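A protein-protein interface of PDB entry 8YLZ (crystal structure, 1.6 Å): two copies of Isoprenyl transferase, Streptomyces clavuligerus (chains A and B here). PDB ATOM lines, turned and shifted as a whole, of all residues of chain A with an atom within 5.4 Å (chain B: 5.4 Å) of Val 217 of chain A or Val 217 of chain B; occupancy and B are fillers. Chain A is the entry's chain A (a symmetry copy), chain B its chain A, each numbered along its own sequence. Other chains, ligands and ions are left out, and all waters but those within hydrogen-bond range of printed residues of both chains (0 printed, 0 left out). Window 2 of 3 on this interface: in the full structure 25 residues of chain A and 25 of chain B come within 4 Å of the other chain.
The guanidinium group (NH1) of Arg 218 of chain B is in hydrogen-bond range of the backbone carbonyl oxygen (O) of Val 233 of chain A (3.1 Å). The backbone carbonyl oxygen of Val 233 of chain B lies within hydrogen-bond range of the guanidinium group of Arg 218 of chain A (3.1 Å).
CD1 of Ile 213 of chain A touches CD1 of Ile 213 of chain B, at 3.7 Å. CG2 of Val 217 of chain A touches CG2 of Val 217 of chain B (3.7 Å). Val 217 of chain A touches Val 233 of chain B (CG1 to CG1, 3.6 Å). CG1 of Val 217 of chain B touches CG1 of Val 233 of chain A (3.6 Å).
Printed residues of chain B within 4 Å of Ile 213 of chain A: Ile 213 (3.7 Å). Val 217 of chain A touches just these residues of chain B: Val 217 (3.7 Å) and Val 233 (3.6 Å). Printed residues of chain B within 4 Å of Arg 218 of chain A: Val 233. Of the printed residues of chain B, Val 233 of chain A touches Val 217 (3.6 Å) and Arg 218 (3.1 Å). Of the printed residues of chain A, Ile 213 of chain B touches Ile 213 (3.7 Å). Val 217 of chain B touches two residues of chain A. The nearest residue of chain B that does not touch Val 217 of chain A is Val 238 of chain B (4.2 Å). The nearest printed residue of chain A that does not touch Arg 218 of chain B is Val 238 of chain A (6.9 Å).
Along chain A the printed residues that touch a printed residue of chain B span positions 213 to 233. Among the printed residues, 6 pairs touch across the chains. Among the printed residues, no Asp or Glu carboxylate lies within 4 Å of a Lys or Arg side-chain nitrogen of the other chain.
Ile 213 of chain A touches its own counterpart, Ile 213 of chain B. Val 217 of chain B touches its own counterpart, Val 217 of chain A. Val 217 of chain A touches Val 233 of chain B, and with the chains exchanged Val 233 of chain A touches Val 217 of chain B. Arg 218 of chain A touches Val 233 of chain B, and with the chains exchanged Val 233 of chain A touches Arg 218 of chain B. Of the 6 pairs that touch across the chains among the printed residues, 6 have their exchanged pair printed and touching as well.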
ATOM      1  N   ILE A 213     -18.326   8.206   3.825  1.00  0.00           N
ATOM      2  CA  ILE A 213     -18.205   8.351   2.377  1.00  0.00           C
ATOM      3  C   ILE A 213     -19.218   9.361   1.868  1.00  0.00           C
ATOM      4  O   ILE A 213     -18.895  10.241   1.065  1.00  0.00           O
ATOM      5  CB  ILE A 213     -18.378   6.986   1.688  1.00  0.00           C
ATOM      6  CG1 ILE A 213     -17.231   6.050   2.066  1.00  0.00           C
ATOM      7  CG2 ILE A 213     -18.534   7.142   0.153  1.00  0.00           C
ATOM      8  CD1 ILE A 213     -17.407   4.622   1.543  1.00  0.00           C
ATOM      9  N   ALA A 214     -20.469   9.247   2.332  1.00  0.00           N
ATOM     10  CA  ALA A 214     -21.496  10.200   1.917  1.00  0.00           C
ATOM     11  C   ALA A 214     -21.125  11.640   2.264  1.00  0.00           C
ATOM     12  O   ALA A 214     -21.485  12.562   1.526  1.00  0.00           O
ATOM     13  CB  ALA A 214     -22.836   9.830   2.547  1.00  0.00           C
ATOM     14  N   GLY A 215     -20.411  11.857   3.375  1.00  0.00           N
ATOM     15  CA  GLY A 215     -19.962  13.203   3.710  1.00  0.00           C
ATOM     16  C   GLY A 215     -18.978  13.786   2.713  1.00  0.00           C
ATOM     17  O   GLY A 215     -18.913  15.008   2.535  1.00  0.00           O
ATOM     18  N   ALA A 216     -18.172  12.940   2.079  1.00  0.00           N
ATOM     19  CA  ALA A 216     -17.284  13.445   1.039  1.00  0.00           C
ATOM     20  C   ALA A 216     -18.069  14.025  -0.138  1.00  0.00           C
ATOM     21  O   ALA A 216     -17.588  14.941  -0.811  1.00  0.00           O
ATOM     22  CB  ALA A 216     -16.336  12.336   0.581  1.00  0.00           C
ATOM     23  N   VAL A 217     -19.279  13.518  -0.393  1.00  0.00           N
ATOM     24  CA  VAL A 217     -20.118  14.069  -1.458  1.00  0.00           C
ATOM     25  C   VAL A 217     -20.658  15.435  -1.052  1.00  0.00           C
ATOM     26  O   VAL A 217     -20.549  16.419  -1.792  1.00  0.00           O
ATOM     27  CB  VAL A 217     -21.260  13.089  -1.786  1.00  0.00           C
ATOM     28  CG1 VAL A 217     -22.449  13.828  -2.393  1.00  0.00           C
ATOM     29  CG2 VAL A 217     -20.779  11.973  -2.687  1.00  0.00           C
ATOM     30  N   ARG A 218     -21.257  15.513   0.132  1.00  0.00           N
ATOM     31  CA  ARG A 218     -21.731  16.792   0.644  1.00  0.00           C
ATOM     32  C   ARG A 218     -20.604  17.815   0.730  1.00  0.00           C
ATOM     33  O   ARG A 218     -20.829  19.010   0.493  1.00  0.00           O
ATOM     34  CB  ARG A 218     -22.393  16.563   2.002  1.00  0.00           C
ATOM     35  CG  ARG A 218     -23.781  15.952   1.868  1.00  0.00           C
ATOM     36  CD  ARG A 218     -24.445  15.623   3.193  1.00  0.00           C
ATOM     37  NE  ARG A 218     -23.712  14.620   3.960  1.00  0.00           N
ATOM     38  CZ  ARG A 218     -24.137  13.377   4.152  1.00  0.00           C
ATOM     39  NH1 ARG A 218     -25.267  12.942   3.617  1.00  0.00           N
ATOM     40  NH2 ARG A 218     -23.408  12.549   4.897  1.00  0.00           N
ATOM     41  N   GLY A 219     -19.380  17.368   1.030  1.00  0.00           N
ATOM     42  CA  GLY A 219     -18.262  18.293   1.085  1.00  0.00           C
ATOM     43  C   GLY A 219     -17.889  18.855  -0.273  1.00  0.00           C
ATOM     44  O   GLY A 219     -17.642  20.058  -0.408  1.00  0.00           O
ATOM     45  N   LEU A 220     -17.826  18.001  -1.294  1.00  0.00           N
ATOM     46  CA  LEU A 220     -17.499  18.498  -2.630  1.00  0.00           C
ATOM     47  C   LEU A 220     -18.581  19.432  -3.155  1.00  0.00           C
ATOM     48  O   LEU A 220     -18.279  20.434  -3.815  1.00  0.00           O
ATOM     49  CB  LEU A 220     -17.285  17.333  -3.592  1.00  0.00           C
ATOM     50  CG  LEU A 220     -15.925  16.654  -3.435  1.00  0.00           C
ATOM     51  CD1 LEU A 220     -15.881  15.333  -4.161  1.00  0.00           C
ATOM     52  CD2 LEU A 220     -14.838  17.566  -3.982  1.00  0.00           C
ATOM     53  N   LEU A 221     -19.845  19.116  -2.870  1.00  0.00           N
ATOM     54  CA  LEU A 221     -20.949  19.975  -3.277  1.00  0.00           C
ATOM     55  C   LEU A 221     -20.769  21.388  -2.738  1.00  0.00           C
ATOM     56  O   LEU A 221     -20.796  22.365  -3.498  1.00  0.00           O
ATOM     57  CB  LEU A 221     -22.270  19.365  -2.797  1.00  0.00           C
ATOM     58  CG  LEU A 221     -23.608  19.720  -3.450  1.00  0.00           C
ATOM     59  CD1 LEU A 221     -23.563  19.529  -4.960  1.00  0.00           C
ATOM     60  CD2 LEU A 221     -24.726  18.885  -2.835  1.00  0.00           C
ATOM     61  N   ARG A 222     -20.561  21.519  -1.426  1.00  0.00           N
ATOM     62  CA  ARG A 222     -20.433  22.846  -0.831  1.00  0.00           C
ATOM     63  C   ARG A 222     -19.177  23.571  -1.298  1.00  0.00           C
ATOM     64  O   ARG A 222     -19.109  24.801  -1.190  1.00  0.00           O
ATOM     65  CB  ARG A 222     -20.447  22.751   0.698  1.00  0.00           C
ATOM     66  CG  ARG A 222     -21.597  21.927   1.271  1.00  0.00           C
ATOM     67  CD  ARG A 222     -22.921  22.174   0.546  1.00  0.00           C
ATOM     68  NE  ARG A 222     -23.877  21.098   0.790  1.00  0.00           N
ATOM     69  CZ  ARG A 222     -25.054  20.983   0.187  1.00  0.00           C
ATOM     70  NH1 ARG A 222     -25.477  21.885  -0.685  1.00  0.00           N
ATOM     71  NH2 ARG A 222     -25.826  19.937   0.466  1.00  0.00           N
ATOM     72  N   VAL A 233     -13.339  15.596 -10.831  1.00  0.00           N
ATOM     73  CA  VAL A 233     -13.138  15.057  -9.481  1.00  0.00           C
ATOM     74  C   VAL A 233     -12.225  13.830  -9.505  1.00  0.00           C
ATOM     75  O   VAL A 233     -12.456  12.866 -10.239  1.00  0.00           O
ATOM     76  CB  VAL A 233     -14.486  14.741  -8.802  1.00  0.00           C
ATOM     77  CG1 VAL A 233     -15.307  13.797  -9.657  1.00  0.00           C
ATOM     78  CG2 VAL A 233     -14.263  14.139  -7.416  1.00  0.00           C
ATOM     79  N   VAL A 238     -11.970  13.093  -3.322  1.00  0.00           N
ATOM     80  CA  VAL A 238     -12.913  12.418  -2.436  1.00  0.00           C
ATOM     81  C   VAL A 238     -12.295  12.253  -1.053  1.00  0.00           C
ATOM     82  O   VAL A 238     -12.917  12.548  -0.024  1.00  0.00           O
ATOM     83  CB  VAL A 238     -13.334  11.064  -3.040  1.00  0.00           C
ATOM     84  CG1 VAL A 238     -14.175  10.286  -2.047  1.00  0.00           C
ATOM     85  CG2 VAL A 238     -14.093  11.292  -4.366  1.00  0.00           C
ATOM     86  N   ILE B 213     -15.820   4.173  -5.666  1.00  0.00           N
ATOM     87  CA  ILE B 213     -16.444   5.215  -4.855  1.00  0.00           C
ATOM     88  C   ILE B 213     -16.419   6.538  -5.599  1.00  0.00           C
ATOM     89  O   ILE B 213     -17.420   7.259  -5.654  1.00  0.00           O
ATOM     90  CB  ILE B 213     -15.739   5.323  -3.492  1.00  0.00           C
ATOM     91  CG1 ILE B 213     -15.947   4.046  -2.681  1.00  0.00           C
ATOM     92  CG2 ILE B 213     -16.186   6.594  -2.722  1.00  0.00           C
ATOM     93  CD1 ILE B 213     -15.153   4.011  -1.373  1.00  0.00           C
ATOM     94  N   ALA B 214     -15.264   6.880  -6.185  1.00  0.00           N
ATOM     95  CA  ALA B 214     -15.167   8.122  -6.948  1.00  0.00           C
ATOM     96  C   ALA B 214     -16.170   8.177  -8.097  1.00  0.00           C
ATOM     97  O   ALA B 214     -16.660   9.259  -8.435  1.00  0.00           O
ATOM     98  CB  ALA B 214     -13.746   8.301  -7.475  1.00  0.00           C
ATOM     99  N   GLY B 215     -16.491   7.030  -8.710  1.00  0.00           N
ATOM    100  CA  GLY B 215     -17.504   7.015  -9.758  1.00  0.00           C
ATOM    101  C   GLY B 215     -18.892   7.388  -9.275  1.00  0.00           C
ATOM    102  O   GLY B 215     -19.702   7.924 -10.040  1.00  0.00           O
ATOM    103  N   ALA B 216     -19.210   7.079  -8.021  1.00  0.00           N
ATOM    104  CA  ALA B 216     -20.495   7.510  -7.484  1.00  0.00           C
ATOM    105  C   ALA B 216     -20.601   9.036  -7.436  1.00  0.00           C
ATOM    106  O   ALA B 216     -21.701   9.583  -7.549  1.00  0.00           O
ATOM    107  CB  ALA B 216     -20.713   6.896  -6.101  1.00  0.00           C
ATOM    108  N   VAL B 217     -19.473   9.736  -7.285  1.00  0.00           N
ATOM    109  CA  VAL B 217     -19.487  11.199  -7.302  1.00  0.00           C
ATOM    110  C   VAL B 217     -19.742  11.710  -8.715  1.00  0.00           C
ATOM    111  O   VAL B 217     -20.621  12.546  -8.951  1.00  0.00           O
ATOM    112  CB  VAL B 217     -18.160  11.743  -6.740  1.00  0.00           C
ATOM    113  CG1 VAL B 217     -17.876  13.142  -7.280  1.00  0.00           C
ATOM    114  CG2 VAL B 217     -18.158  11.720  -5.227  1.00  0.00           C
ATOM    115  N   ARG B 218     -18.967  11.218  -9.677  1.00  0.00           N
ATOM    116  CA  ARG B 218     -19.189  11.581 -11.070  1.00  0.00           C
ATOM    117  C   ARG B 218     -20.604  11.239 -11.522  1.00  0.00           C
ATOM    118  O   ARG B 218     -21.197  11.976 -12.321  1.00  0.00           O
ATOM    119  CB  ARG B 218     -18.136  10.887 -11.933  1.00  0.00           C
ATOM    120  CG  ARG B 218     -16.776  11.564 -11.834  1.00  0.00           C
ATOM    121  CD  ARG B 218     -15.674  10.859 -12.604  1.00  0.00           C
ATOM    122  NE  ARG B 218     -15.411   9.511 -12.109  1.00  0.00           N
ATOM    123  CZ  ARG B 218     -14.313   9.164 -11.448  1.00  0.00           C
ATOM    124  NH1 ARG B 218     -13.374  10.051 -11.155  1.00  0.00           N
ATOM    125  NH2 ARG B 218     -14.154   7.898 -11.069  1.00  0.00           N
ATOM    126  N   GLY B 219     -21.178  10.151 -10.997  1.00  0.00           N
ATOM    127  CA  GLY B 219     -22.539   9.800 -11.361  1.00  0.00           C
ATOM    128  C   GLY B 219     -23.567  10.783 -10.832  1.00  0.00           C
ATOM    129  O   GLY B 219     -24.489  11.176 -11.553  1.00  0.00           O
ATOM    130  N   LEU B 220     -23.438  11.184  -9.567  1.00  0.00           N
ATOM    131  CA  LEU B 220     -24.385  12.153  -9.018  1.00  0.00           C
ATOM    132  C   LEU B 220     -24.269  13.501  -9.717  1.00  0.00           C
ATOM    133  O   LEU B 220     -25.281  14.172  -9.956  1.00  0.00           O
ATOM    134  CB  LEU B 220     -24.173  12.310  -7.515  1.00  0.00           C
ATOM    135  CG  LEU B 220     -24.760  11.164  -6.692  1.00  0.00           C
ATOM    136  CD1 LEU B 220     -24.255  11.190  -5.272  1.00  0.00           C
ATOM    137  CD2 LEU B 220     -26.277  11.268  -6.691  1.00  0.00           C
ATOM    138  N   LEU B 221     -23.044  13.907 -10.052  1.00  0.00           N
ATOM    139  CA  LEU B 221     -22.832  15.153 -10.774  1.00  0.00           C
ATOM    140  C   LEU B 221     -23.617  15.168 -12.080  1.00  0.00           C
ATOM    141  O   LEU B 221     -24.395  16.093 -12.341  1.00  0.00           O
ATOM    142  CB  LEU B 221     -21.333  15.343 -11.030  1.00  0.00           C
ATOM    143  CG  LEU B 221     -20.729  16.722 -11.307  1.00  0.00           C
ATOM    144  CD1 LEU B 221     -21.121  17.732 -10.236  1.00  0.00           C
ATOM    145  CD2 LEU B 221     -19.212  16.615 -11.416  1.00  0.00           C
ATOM    146  N   ARG B 222     -23.443  14.135 -12.909  1.00  0.00           N
ATOM    147  CA  ARG B 222     -24.121  14.108 -14.200  1.00  0.00           C
ATOM    148  C   ARG B 222     -25.633  13.988 -14.058  1.00  0.00           C
ATOM    149  O   ARG B 222     -26.360  14.316 -15.003  1.00  0.00           O
ATOM    150  CB  ARG B 222     -23.581  12.963 -15.064  1.00  0.00           C
ATOM    151  CG  ARG B 222     -22.060  12.908 -15.166  1.00  0.00           C
ATOM    152  CD  ARG B 222     -21.426  14.293 -15.317  1.00  0.00           C
ATOM    153  NE  ARG B 222     -20.008  14.276 -14.973  1.00  0.00           N
ATOM    154  CZ  ARG B 222     -19.239  15.355 -14.888  1.00  0.00           C
ATOM    155  NH1 ARG B 222     -19.710  16.563 -15.149  1.00  0.00           N
ATOM    156  NH2 ARG B 222     -17.964  15.216 -14.531  1.00  0.00           N
ATOM    157  N   VAL B 233     -28.394  14.698  -0.626  1.00  0.00           N
ATOM    158  CA  VAL B 233     -27.817  13.399  -0.989  1.00  0.00           C
ATOM    159  C   VAL B 233     -27.805  12.444   0.206  1.00  0.00           C
ATOM    160  O   VAL B 233     -27.302  12.765   1.285  1.00  0.00           O
ATOM    161  CB  VAL B 233     -26.405  13.565  -1.588  1.00  0.00           C
ATOM    162  CG1 VAL B 233     -25.506  14.322  -0.633  1.00  0.00           C
ATOM    163  CG2 VAL B 233     -25.797  12.204  -1.920  1.00  0.00           C
ATOM    164  N   VAL B 238     -25.658   7.506  -2.931  1.00  0.00           N
ATOM    165  CA  VAL B 238     -24.280   7.158  -3.268  1.00  0.00           C
ATOM    166  C   VAL B 238     -24.224   5.729  -3.795  1.00  0.00           C
ATOM    167  O   VAL B 238     -23.605   5.442  -4.829  1.00  0.00           O
ATOM    168  CB  VAL B 238     -23.368   7.351  -2.041  1.00  0.00           C
ATOM    169  CG1 VAL B 238     -21.976   6.828  -2.336  1.00  0.00           C
ATOM    170  CG2 VAL B 238     -23.337   8.842  -1.637  1.00  0.00           C
